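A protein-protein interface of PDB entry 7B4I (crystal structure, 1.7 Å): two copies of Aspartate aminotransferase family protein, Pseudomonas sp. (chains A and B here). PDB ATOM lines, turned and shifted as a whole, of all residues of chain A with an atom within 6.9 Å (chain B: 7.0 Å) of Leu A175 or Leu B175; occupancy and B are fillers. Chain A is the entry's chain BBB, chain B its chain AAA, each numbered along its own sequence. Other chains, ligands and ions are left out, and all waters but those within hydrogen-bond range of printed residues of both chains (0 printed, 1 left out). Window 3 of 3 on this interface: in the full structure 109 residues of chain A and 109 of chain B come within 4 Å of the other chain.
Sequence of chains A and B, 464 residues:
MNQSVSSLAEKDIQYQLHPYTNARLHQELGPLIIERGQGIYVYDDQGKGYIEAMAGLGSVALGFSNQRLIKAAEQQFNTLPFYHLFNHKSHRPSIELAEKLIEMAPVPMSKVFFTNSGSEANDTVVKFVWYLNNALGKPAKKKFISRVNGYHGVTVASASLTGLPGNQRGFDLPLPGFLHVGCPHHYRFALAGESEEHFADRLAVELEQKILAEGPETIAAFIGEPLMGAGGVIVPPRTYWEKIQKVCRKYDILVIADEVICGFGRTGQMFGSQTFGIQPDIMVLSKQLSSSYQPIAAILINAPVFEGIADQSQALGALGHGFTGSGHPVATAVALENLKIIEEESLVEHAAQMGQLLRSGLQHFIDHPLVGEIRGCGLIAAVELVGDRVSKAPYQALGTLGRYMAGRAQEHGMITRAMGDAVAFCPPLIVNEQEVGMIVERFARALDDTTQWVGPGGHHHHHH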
ATOM      1  N   TRP A 130      31.897 -23.639 -38.795  1.00  0.00           N
ATOM      2  CA  TRP A 130      32.806 -23.702 -37.621  1.00  0.00           C
ATOM      3  C   TRP A 130      33.534 -25.055 -37.631  1.00  0.00           C
ATOM      4  O   TRP A 130      34.774 -25.112 -37.440  1.00  0.00           O
ATOM      5  CB  TRP A 130      32.064 -23.480 -36.313  1.00  0.00           C
ATOM      6  CG  TRP A 130      31.483 -22.111 -36.134  1.00  0.00           C
ATOM      7  CD1 TRP A 130      31.735 -21.015 -36.896  1.00  0.00           C
ATOM      8  CD2 TRP A 130      30.609 -21.676 -35.087  1.00  0.00           C
ATOM      9  NE1 TRP A 130      31.061 -19.936 -36.400  1.00  0.00           N
ATOM     10  CE2 TRP A 130      30.381 -20.297 -35.281  1.00  0.00           C
ATOM     11  CE3 TRP A 130      29.973 -22.307 -34.019  1.00  0.00           C
ATOM     12  CZ2 TRP A 130      29.549 -19.551 -34.447  1.00  0.00           C
ATOM     13  CZ3 TRP A 130      29.176 -21.569 -33.174  1.00  0.00           C
ATOM     14  CH2 TRP A 130      28.956 -20.209 -33.397  1.00  0.00           C
ATOM     15  N   VAL A 156      18.683 -18.800 -31.888  1.00  0.00           N
ATOM     16  CA  VAL A 156      19.697 -17.878 -31.292  1.00  0.00           C
ATOM     17  C   VAL A 156      20.755 -17.522 -32.352  1.00  0.00           C
ATOM     18  O   VAL A 156      21.012 -16.324 -32.571  1.00  0.00           O
ATOM     19  CB  VAL A 156      20.282 -18.476 -30.010  1.00  0.00           C
ATOM     20  CG1 VAL A 156      21.479 -17.666 -29.532  1.00  0.00           C
ATOM     21  CG2 VAL A 156      19.222 -18.610 -28.923  1.00  0.00           C
ATOM     22  N   ALA A 157      21.314 -18.490 -33.078  1.00  0.00           N
ATOM     23  CA  ALA A 157      22.327 -18.226 -34.124  1.00  0.00           C
ATOM     24  C   ALA A 157      21.716 -17.652 -35.411  1.00  0.00           C
ATOM     25  O   ALA A 157      22.250 -16.666 -35.943  1.00  0.00           O
ATOM     26  CB  ALA A 157      23.120 -19.472 -34.399  1.00  0.00           C
ATOM     27  N   ALA A 159      18.890 -16.011 -35.900  1.00  0.00           N
ATOM     28  CA  ALA A 159      18.366 -14.653 -35.594  1.00  0.00           C
ATOM     29  C   ALA A 159      19.542 -13.678 -35.408  1.00  0.00           C
ATOM     30  O   ALA A 159      19.323 -12.459 -35.571  1.00  0.00           O
ATOM     31  CB  ALA A 159      17.461 -14.675 -34.388  1.00  0.00           C
ATOM     32  N   SER A 160      20.744 -14.179 -35.087  1.00  0.00           N
ATOM     33  CA  SER A 160      21.987 -13.348 -35.054  1.00  0.00           C
ATOM     34  C   SER A 160      22.410 -13.000 -36.483  1.00  0.00           C
ATOM     35  O   SER A 160      22.842 -11.860 -36.729  1.00  0.00           O
ATOM     36  CB  SER A 160      23.092 -14.017 -34.275  1.00  0.00           C
ATOM     37  OG  SER A 160      22.739 -14.119 -32.914  1.00  0.00           O
ATOM     38  N   LEU A 161      22.244 -13.925 -37.435  1.00  0.00           N
ATOM     39  CA  LEU A 161      22.442 -13.673 -38.877  1.00  0.00           C
ATOM     40  C   LEU A 161      21.382 -12.675 -39.373  1.00  0.00           C
ATOM     41  O   LEU A 161      21.732 -11.775 -40.122  1.00  0.00           O
ATOM     42  CB  LEU A 161      22.359 -14.988 -39.654  1.00  0.00           C
ATOM     43  CG  LEU A 161      23.481 -15.989 -39.383  1.00  0.00           C
ATOM     44  CD1 LEU A 161      23.149 -17.317 -40.037  1.00  0.00           C
ATOM     45  CD2 LEU A 161      24.821 -15.460 -39.878  1.00  0.00           C
ATOM     46  N   GLN A 168      15.749  -9.210 -33.004  1.00  0.00           N
ATOM     47  CA  GLN A 168      16.915  -9.108 -32.079  1.00  0.00           C
ATOM     48  C   GLN A 168      16.543  -8.355 -30.793  1.00  0.00           C
ATOM     49  O   GLN A 168      17.000  -8.784 -29.714  1.00  0.00           O
ATOM     50  CB  GLN A 168      18.087  -8.486 -32.829  1.00  0.00           C
ATOM     51  CG  GLN A 168      18.471  -9.285 -34.063  1.00  0.00           C
ATOM     52  CD  GLN A 168      19.761  -8.839 -34.697  1.00  0.00           C
ATOM     53  OE1 GLN A 168      20.073  -7.649 -34.774  1.00  0.00           O
ATOM     54  NE2 GLN A 168      20.494  -9.796 -35.231  1.00  0.00           N
ATOM     55  N   ASP A 172      18.687 -10.253 -26.632  1.00  0.00           N
ATOM     56  CA  ASP A 172      20.163 -10.177 -26.438  1.00  0.00           C
ATOM     57  C   ASP A 172      20.922 -10.672 -27.680  1.00  0.00           C
ATOM     58  O   ASP A 172      21.950 -11.341 -27.497  1.00  0.00           O
ATOM     59  CB  ASP A 172      20.610 -10.985 -25.217  1.00  0.00           C
ATOM     60  CG  ASP A 172      19.982 -10.580 -23.892  1.00  0.00           C
ATOM     61  OD1 ASP A 172      19.424  -9.481 -23.807  1.00  0.00           O
ATOM     62  OD2 ASP A 172      20.052 -11.390 -22.951  1.00  0.00           O
ATOM     63  N   LEU A 173      20.456 -10.350 -28.890  1.00  0.00           N
ATOM     64  CA  LEU A 173      21.094 -10.724 -30.172  1.00  0.00           C
ATOM     65  C   LEU A 173      21.542  -9.458 -30.886  1.00  0.00           C
ATOM     66  O   LEU A 173      20.986  -8.390 -30.646  1.00  0.00           O
ATOM     67  CB  LEU A 173      20.079 -11.512 -31.019  1.00  0.00           C
ATOM     68  CG  LEU A 173      19.540 -12.777 -30.360  1.00  0.00           C
ATOM     69  CD1 LEU A 173      18.547 -13.485 -31.277  1.00  0.00           C
ATOM     70  CD2 LEU A 173      20.657 -13.731 -29.964  1.00  0.00           C
ATOM     71  N   PRO A 174      22.525  -9.520 -31.813  1.00  0.00           N
ATOM     72  CA  PRO A 174      23.193 -10.769 -32.178  1.00  0.00           C
ATOM     73  C   PRO A 174      24.216 -11.272 -31.155  1.00  0.00           C
ATOM     74  O   PRO A 174      24.731 -10.472 -30.360  1.00  0.00           O
ATOM     75  CB  PRO A 174      23.930 -10.404 -33.458  1.00  0.00           C
ATOM     76  CG  PRO A 174      24.243  -8.928 -33.293  1.00  0.00           C
ATOM     77  CD  PRO A 174      23.023  -8.374 -32.590  1.00  0.00           C
ATOM     78  N   LEU A 175      24.491 -12.572 -31.194  1.00  0.00           N
ATOM     79  CA  LEU A 175      25.685 -13.170 -30.539  1.00  0.00           C
ATOM     80  C   LEU A 175      26.931 -12.450 -31.042  1.00  0.00           C
ATOM     81  O   LEU A 175      26.978 -11.958 -32.166  1.00  0.00           O
ATOM     82  CB  LEU A 175      25.791 -14.660 -30.884  1.00  0.00           C
ATOM     83  CG  LEU A 175      24.743 -15.601 -30.293  1.00  0.00           C
ATOM     84  CD1 LEU A 175      25.044 -17.027 -30.743  1.00  0.00           C
ATOM     85  CD2 LEU A 175      24.682 -15.523 -28.783  1.00  0.00           C
ATOM     86  N   PRO A 176      28.031 -12.448 -30.259  1.00  0.00           N
ATOM     87  CA  PRO A 176      29.338 -12.067 -30.785  1.00  0.00           C
ATOM     88  C   PRO A 176      29.731 -12.898 -32.015  1.00  0.00           C
ATOM     89  O   PRO A 176      29.461 -14.082 -32.028  1.00  0.00           O
ATOM     90  CB  PRO A 176      30.329 -12.379 -29.640  1.00  0.00           C
ATOM     91  CG  PRO A 176      29.488 -12.577 -28.394  1.00  0.00           C
ATOM     92  CD  PRO A 176      28.060 -12.827 -28.847  1.00  0.00           C
ATOM     93  N   GLY A 177      30.375 -12.271 -32.998  1.00  0.00           N
ATOM     94  CA  GLY A 177      30.953 -12.936 -34.176  1.00  0.00           C
ATOM     95  C   GLY A 177      29.964 -13.007 -35.327  1.00  0.00           C
ATOM     96  O   GLY A 177      30.274 -13.632 -36.333  1.00  0.00           O
ATOM     97  N   PHE A 178      28.808 -12.364 -35.169  1.00  0.00           N
ATOM     98  CA  PHE A 178      27.784 -12.193 -36.226  1.00  0.00           C
ATOM     99  C   PHE A 178      27.705 -10.701 -36.547  1.00  0.00           C
ATOM    100  O   PHE A 178      27.094  -9.952 -35.772  1.00  0.00           O
ATOM    101  CB  PHE A 178      26.446 -12.781 -35.770  1.00  0.00           C
ATOM    102  CG  PHE A 178      26.508 -14.267 -35.532  1.00  0.00           C
ATOM    103  CD1 PHE A 178      26.973 -14.780 -34.333  1.00  0.00           C
ATOM    104  CD2 PHE A 178      26.099 -15.149 -36.518  1.00  0.00           C
ATOM    105  CE1 PHE A 178      27.051 -16.151 -34.127  1.00  0.00           C
ATOM    106  CE2 PHE A 178      26.170 -16.516 -36.305  1.00  0.00           C
ATOM    107  CZ  PHE A 178      26.631 -17.016 -35.115  1.00  0.00           C
ATOM    108  N   LEU A 179      28.363 -10.318 -37.636  1.00  0.00           N
ATOM    109  CA  LEU A 179      28.573  -8.912 -38.043  1.00  0.00           C
ATOM    110  C   LEU A 179      27.588  -8.572 -39.161  1.00  0.00           C
ATOM    111  O   LEU A 179      27.213  -9.482 -39.932  1.00  0.00           O
ATOM    112  CB  LEU A 179      30.009  -8.758 -38.537  1.00  0.00           C
ATOM    113  CG  LEU A 179      31.076  -9.334 -37.608  1.00  0.00           C
ATOM    114  CD1 LEU A 179      32.436  -9.218 -38.267  1.00  0.00           C
ATOM    115  CD2 LEU A 179      31.042  -8.645 -36.253  1.00  0.00           C
ATOM    116  N   HIS A 180      27.204  -7.299 -39.268  1.00  0.00           N
ATOM    117  CA  HIS A 180      26.194  -6.853 -40.259  1.00  0.00           C
ATOM    118  C   HIS A 180      26.732  -5.673 -41.055  1.00  0.00           C
ATOM    119  O   HIS A 180      27.259  -4.741 -40.426  1.00  0.00           O
ATOM    120  CB  HIS A 180      24.884  -6.518 -39.553  1.00  0.00           C
ATOM    121  CG  HIS A 180      24.276  -7.705 -38.899  1.00  0.00           C
ATOM    122  ND1 HIS A 180      24.702  -8.155 -37.677  1.00  0.00           N
ATOM    123  CD2 HIS A 180      23.291  -8.540 -39.308  1.00  0.00           C
ATOM    124  CE1 HIS A 180      24.008  -9.235 -37.348  1.00  0.00           C
ATOM    125  NE2 HIS A 180      23.109  -9.468 -38.321  1.00  0.00           N
ATOM    126  N   TRP B 130      15.336 -15.273 -21.952  1.00  0.00           N
ATOM    127  CA  TRP B 130      16.115 -14.014 -22.106  1.00  0.00           C
ATOM    128  C   TRP B 130      15.155 -12.838 -22.298  1.00  0.00           C
ATOM    129  O   TRP B 130      15.330 -11.782 -21.652  1.00  0.00           O
ATOM    130  CB  TRP B 130      17.105 -14.099 -23.270  1.00  0.00           C
ATOM    131  CG  TRP B 130      18.222 -15.075 -23.087  1.00  0.00           C
ATOM    132  CD1 TRP B 130      18.570 -15.742 -21.948  1.00  0.00           C
ATOM    133  CD2 TRP B 130      19.195 -15.443 -24.073  1.00  0.00           C
ATOM    134  NE1 TRP B 130      19.672 -16.520 -22.173  1.00  0.00           N
ATOM    135  CE2 TRP B 130      20.086 -16.349 -23.461  1.00  0.00           C
ATOM    136  CE3 TRP B 130      19.389 -15.118 -25.418  1.00  0.00           C
ATOM    137  CZ2 TRP B 130      21.158 -16.917 -24.147  1.00  0.00           C
ATOM    138  CZ3 TRP B 130      20.449 -15.679 -26.096  1.00  0.00           C
ATOM    139  CH2 TRP B 130      21.315 -16.575 -25.471  1.00  0.00           C
ATOM    140  N   VAL B 156      22.881 -24.253 -32.287  1.00  0.00           N
ATOM    141  CA  VAL B 156      24.023 -23.621 -31.572  1.00  0.00           C
ATOM    142  C   VAL B 156      23.664 -23.483 -30.083  1.00  0.00           C
ATOM    143  O   VAL B 156      24.466 -23.913 -29.219  1.00  0.00           O
ATOM    144  CB  VAL B 156      24.406 -22.290 -32.239  1.00  0.00           C
ATOM    145  CG1 VAL B 156      25.419 -21.542 -31.379  1.00  0.00           C
ATOM    146  CG2 VAL B 156      24.947 -22.516 -33.641  1.00  0.00           C
ATOM    147  N   ALA B 157      22.471 -22.981 -29.754  1.00  0.00           N
ATOM    148  CA  ALA B 157      22.045 -22.794 -28.351  1.00  0.00           C
ATOM    149  C   ALA B 157      21.633 -24.122 -27.695  1.00  0.00           C
ATOM    150  O   ALA B 157      22.057 -24.396 -26.563  1.00  0.00           O
ATOM    151  CB  ALA B 157      20.962 -21.754 -28.265  1.00  0.00           C
ATOM    152  N   SER B 158      20.793 -24.946 -28.328  1.00  0.00           N
ATOM    153  CA  SER B 158      20.327 -26.178 -27.666  1.00  0.00           C
ATOM    154  C   SER B 158      21.478 -27.189 -27.547  1.00  0.00           C
ATOM    155  O   SER B 158      21.461 -27.953 -26.573  1.00  0.00           O
ATOM    156  CB  SER B 158      19.049 -26.728 -28.293  1.00  0.00           C
ATOM    157  OG  SER B 158      19.226 -27.011 -29.668  1.00  0.00           O
ATOM    158  N   ALA B 159      22.452 -27.214 -28.460  1.00  0.00           N
ATOM    159  CA  ALA B 159      23.642 -28.090 -28.338  1.00  0.00           C
ATOM    160  C   ALA B 159      24.556 -27.556 -27.218  1.00  0.00           C
ATOM    161  O   ALA B 159      25.381 -28.351 -26.703  1.00  0.00           O
ATOM    162  CB  ALA B 159      24.390 -28.212 -29.646  1.00  0.00           C
ATOM    163  N   SER B 160      24.435 -26.271 -26.860  1.00  0.00           N
ATOM    164  CA  SER B 160      25.150 -25.689 -25.684  1.00  0.00           C
ATOM    165  C   SER B 160      24.475 -26.190 -24.396  1.00  0.00           C
ATOM    166  O   SER B 160      25.185 -26.481 -23.411  1.00  0.00           O
ATOM    167  CB  SER B 160      25.218 -24.189 -25.770  1.00  0.00           C
ATOM    168  OG  SER B 160      26.010 -23.790 -26.873  1.00  0.00           O
ATOM    169  N   LEU B 161      23.148 -26.339 -24.386  1.00  0.00           N
ATOM    170  CA  LEU B 161      22.397 -26.972 -23.274  1.00  0.00           C
ATOM    171  C   LEU B 161      22.778 -28.453 -23.187  1.00  0.00           C
ATOM    172  O   LEU B 161      23.005 -28.945 -22.071  1.00  0.00           O
ATOM    173  CB  LEU B 161      20.892 -26.825 -23.503  1.00  0.00           C
ATOM    174  CG  LEU B 161      20.327 -25.412 -23.433  1.00  0.00           C
ATOM    175  CD1 LEU B 161      18.874 -25.414 -23.898  1.00  0.00           C
ATOM    176  CD2 LEU B 161      20.409 -24.881 -22.005  1.00  0.00           C
ATOM    177  N   GLN B 168      29.371 -31.294 -29.104  1.00  0.00           N
ATOM    178  CA  GLN B 168      30.097 -30.017 -28.854  1.00  0.00           C
ATOM    179  C   GLN B 168      31.483 -30.028 -29.516  1.00  0.00           C
ATOM    180  O   GLN B 168      31.878 -28.983 -30.074  1.00  0.00           O
ATOM    181  CB  GLN B 168      30.122 -29.768 -27.353  1.00  0.00           C
ATOM    182  CG  GLN B 168      28.732 -29.652 -26.761  1.00  0.00           C
ATOM    183  CD  GLN B 168      28.715 -29.252 -25.307  1.00  0.00           C
ATOM    184  OE1 GLN B 168      29.607 -29.599 -24.539  1.00  0.00           O
ATOM    185  NE2 GLN B 168      27.676 -28.540 -24.906  1.00  0.00           N
ATOM    186  N   ASP B 172      32.840 -25.650 -31.510  1.00  0.00           N
ATOM    187  CA  ASP B 172      33.131 -24.486 -30.630  1.00  0.00           C
ATOM    188  C   ASP B 172      31.999 -24.262 -29.615  1.00  0.00           C
ATOM    189  O   ASP B 172      31.692 -23.094 -29.349  1.00  0.00           O
ATOM    190  CB  ASP B 172      33.358 -23.206 -31.440  1.00  0.00           C
ATOM    191  CG  ASP B 172      34.460 -23.267 -32.486  1.00  0.00           C
ATOM    192  OD1 ASP B 172      35.313 -24.162 -32.403  1.00  0.00           O
ATOM    193  OD2 ASP B 172      34.439 -22.425 -33.404  1.00  0.00           O
ATOM    194  N   LEU B 173      31.409 -25.318 -29.045  1.00  0.00           N
ATOM    195  CA  LEU B 173      30.332 -25.235 -28.030  1.00  0.00           C
ATOM    196  C   LEU B 173      30.826 -25.818 -26.712  1.00  0.00           C
ATOM    197  O   LEU B 173      31.762 -26.619 -26.723  1.00  0.00           O
ATOM    198  CB  LEU B 173      29.119 -26.026 -28.553  1.00  0.00           C
ATOM    199  CG  LEU B 173      28.561 -25.555 -29.888  1.00  0.00           C
ATOM    200  CD1 LEU B 173      27.359 -26.419 -30.286  1.00  0.00           C
ATOM    201  CD2 LEU B 173      28.168 -24.091 -29.832  1.00  0.00           C
ATOM    202  N   PRO B 174      30.214 -25.493 -25.548  1.00  0.00           N
ATOM    203  CA  PRO B 174      29.052 -24.604 -25.469  1.00  0.00           C
ATOM    204  C   PRO B 174      29.381 -23.117 -25.642  1.00  0.00           C
ATOM    205  O   PRO B 174      30.518 -22.719 -25.383  1.00  0.00           O
ATOM    206  CB  PRO B 174      28.515 -24.823 -24.046  1.00  0.00           C
ATOM    207  CG  PRO B 174      29.749 -25.212 -23.248  1.00  0.00           C
ATOM    208  CD  PRO B 174      30.607 -25.993 -24.222  1.00  0.00           C
ATOM    209  N   LEU B 175      28.391 -22.335 -26.079  1.00  0.00           N
ATOM    210  CA  LEU B 175      28.395 -20.854 -25.968  1.00  0.00           C
ATOM    211  C   LEU B 175      28.657 -20.477 -24.510  1.00  0.00           C
ATOM    212  O   LEU B 175      28.301 -21.207 -23.584  1.00  0.00           O
ATOM    213  CB  LEU B 175      27.035 -20.271 -26.376  1.00  0.00           C
ATOM    214  CG  LEU B 175      26.648 -20.353 -27.849  1.00  0.00           C
ATOM    215  CD1 LEU B 175      25.260 -19.746 -28.038  1.00  0.00           C
ATOM    216  CD2 LEU B 175      27.669 -19.676 -28.743  1.00  0.00           C
ATOM    217  N   PRO B 176      29.201 -19.268 -24.256  1.00  0.00           N
ATOM    218  CA  PRO B 176      29.221 -18.727 -22.897  1.00  0.00           C
ATOM    219  C   PRO B 176      27.814 -18.650 -22.289  1.00  0.00           C
ATOM    220  O   PRO B 176      26.906 -18.328 -23.013  1.00  0.00           O
ATOM    221  CB  PRO B 176      29.791 -17.310 -23.056  1.00  0.00           C
ATOM    222  CG  PRO B 176      30.496 -17.319 -24.392  1.00  0.00           C
ATOM    223  CD  PRO B 176      29.787 -18.358 -25.248  1.00  0.00           C
ATOM    224  N   GLY B 177      27.678 -18.901 -20.987  1.00  0.00           N
ATOM    225  CA  GLY B 177      26.427 -18.696 -20.228  1.00  0.00           C
ATOM    226  C   GLY B 177      25.581 -19.957 -20.189  1.00  0.00           C
ATOM    227  O   GLY B 177      24.451 -19.911 -19.675  1.00  0.00           O
ATOM    228  N   PHE B 178      26.119 -21.050 -20.722  1.00  0.00           N
ATOM    229  CA  PHE B 178      25.505 -22.400 -20.679  1.00  0.00           C
ATOM    230  C   PHE B 178      26.405 -23.280 -19.815  1.00  0.00           C
ATOM    231  O   PHE B 178      27.466 -23.724 -20.314  1.00  0.00           O
ATOM    232  CB  PHE B 178      25.317 -22.929 -22.105  1.00  0.00           C
ATOM    233  CG  PHE B 178      24.341 -22.126 -22.920  1.00  0.00           C
ATOM    234  CD1 PHE B 178      24.752 -20.979 -23.585  1.00  0.00           C
ATOM    235  CD2 PHE B 178      22.999 -22.487 -22.981  1.00  0.00           C
ATOM    236  CE1 PHE B 178      23.846 -20.218 -24.308  1.00  0.00           C
ATOM    237  CE2 PHE B 178      22.095 -21.725 -23.703  1.00  0.00           C
ATOM    238  CZ  PHE B 178      22.518 -20.595 -24.368  1.00  0.00           C
ATOM    239  N   LEU B 179      25.993 -23.467 -18.565  1.00  0.00           N
ATOM    240  CA  LEU B 179      26.777 -24.136 -17.500  1.00  0.00           C
ATOM    241  C   LEU B 179      26.256 -25.558 -17.326  1.00  0.00           C
ATOM    242  O   LEU B 179      25.044 -25.779 -17.531  1.00  0.00           O
ATOM    243  CB  LEU B 179      26.614 -23.352 -16.197  1.00  0.00           C
ATOM    244  CG  LEU B 179      26.811 -21.843 -16.324  1.00  0.00           C
ATOM    245  CD1 LEU B 179      26.473 -21.157 -15.012  1.00  0.00           C
ATOM    246  CD2 LEU B 179      28.227 -21.526 -16.775  1.00  0.00           C
ATOM    247  N   HIS B 180      27.126 -26.471 -16.913  1.00  0.00           N
ATOM    248  CA  HIS B 180      26.789 -27.905 -16.755  1.00  0.00           C
ATOM    249  C   HIS B 180      27.185 -28.376 -15.361  1.00  0.00           C
ATOM    250  O   HIS B 180      28.325 -28.114 -14.957  1.00  0.00           O
ATOM    251  CB  HIS B 180      27.448 -28.726 -17.865  1.00  0.00           C
ATOM    252  CG  HIS B 180      26.965 -28.330 -19.218  1.00  0.00           C
ATOM    253  ND1 HIS B 180      27.472 -27.226 -19.878  1.00  0.00           N
ATOM    254  CD2 HIS B 180      26.009 -28.851 -20.019  1.00  0.00           C
ATOM    255  CE1 HIS B 180      26.860 -27.093 -21.040  1.00  0.00           C
ATOM    256  NE2 HIS B 180      25.963 -28.086 -21.156  1.00  0.00           N
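Of the 16 printed residues of chain A, 4 touch a printed residue of chain B. Hydrophobic or aromatic side chains of chain A within 4 Å of the printed part of chain B: Trp A130, Val A156, Ala A157 and Leu A175. Of the 17 printed residues of chain B, 4 touch a printed residue of chain A.
Trp A130 touches Asp B172, but with the chains exchanged Asp A172 does not touch Trp B130 (4.02 Å). Val A156 touches Ala B157, and with the chains exchanged Ala A157 touches Val B156. Leu B175 touches its own counterpart, Leu A175. Positions printed for both chains: 130, 156, 157, 159, 160, 161, 168, 172, 173, 174, 175, 176, 177, 178, 179 and 180.
O of Val B156 lies within hydrogen-bond range of OG of Ser B160, 2.8 Å away. OG of Ser A160 sits at hydrogen-bond distance from O of Val A156, at 2.8 Å. N of Leu B175 is in hydrogen-bond range of OG of Ser B160. The side-chain hydroxyl (OG) of Ser A160 is in hydrogen-bond range of the backbone NH (N) of Leu A175 (2.9 Å).
Of the printed residues of chain B, Val A156 touches Ala B157. Of the printed residues of chain B, Ala A157 touches Val B156. Of chain B, only Leu B175 comes within 4 Å of Leu A175. Of the printed residues of chain A, Val B156 touches Ala A157. Printed residues of chain A within 4 Å of Ala B157: Val A156. Ser B158 touches none of the printed residues of chain A. Of the printed residues of chain A, Asp B172 touches Trp A130. Of chain A, only Leu A175 comes within 4 Å of Leu B175. The nearest residue of chain A that does not touch Leu B175 is Val A156 (4.6 Å).
Among the printed residues, pairs that only touch across the chains: Trp A130 with Asp B172 (3.9 Å), Val A156 with Ala B157 (3.7 Å), Ala A157 with Val B156 (3.6 Å) and Leu A175 with Leu B175 (3.8 Å).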
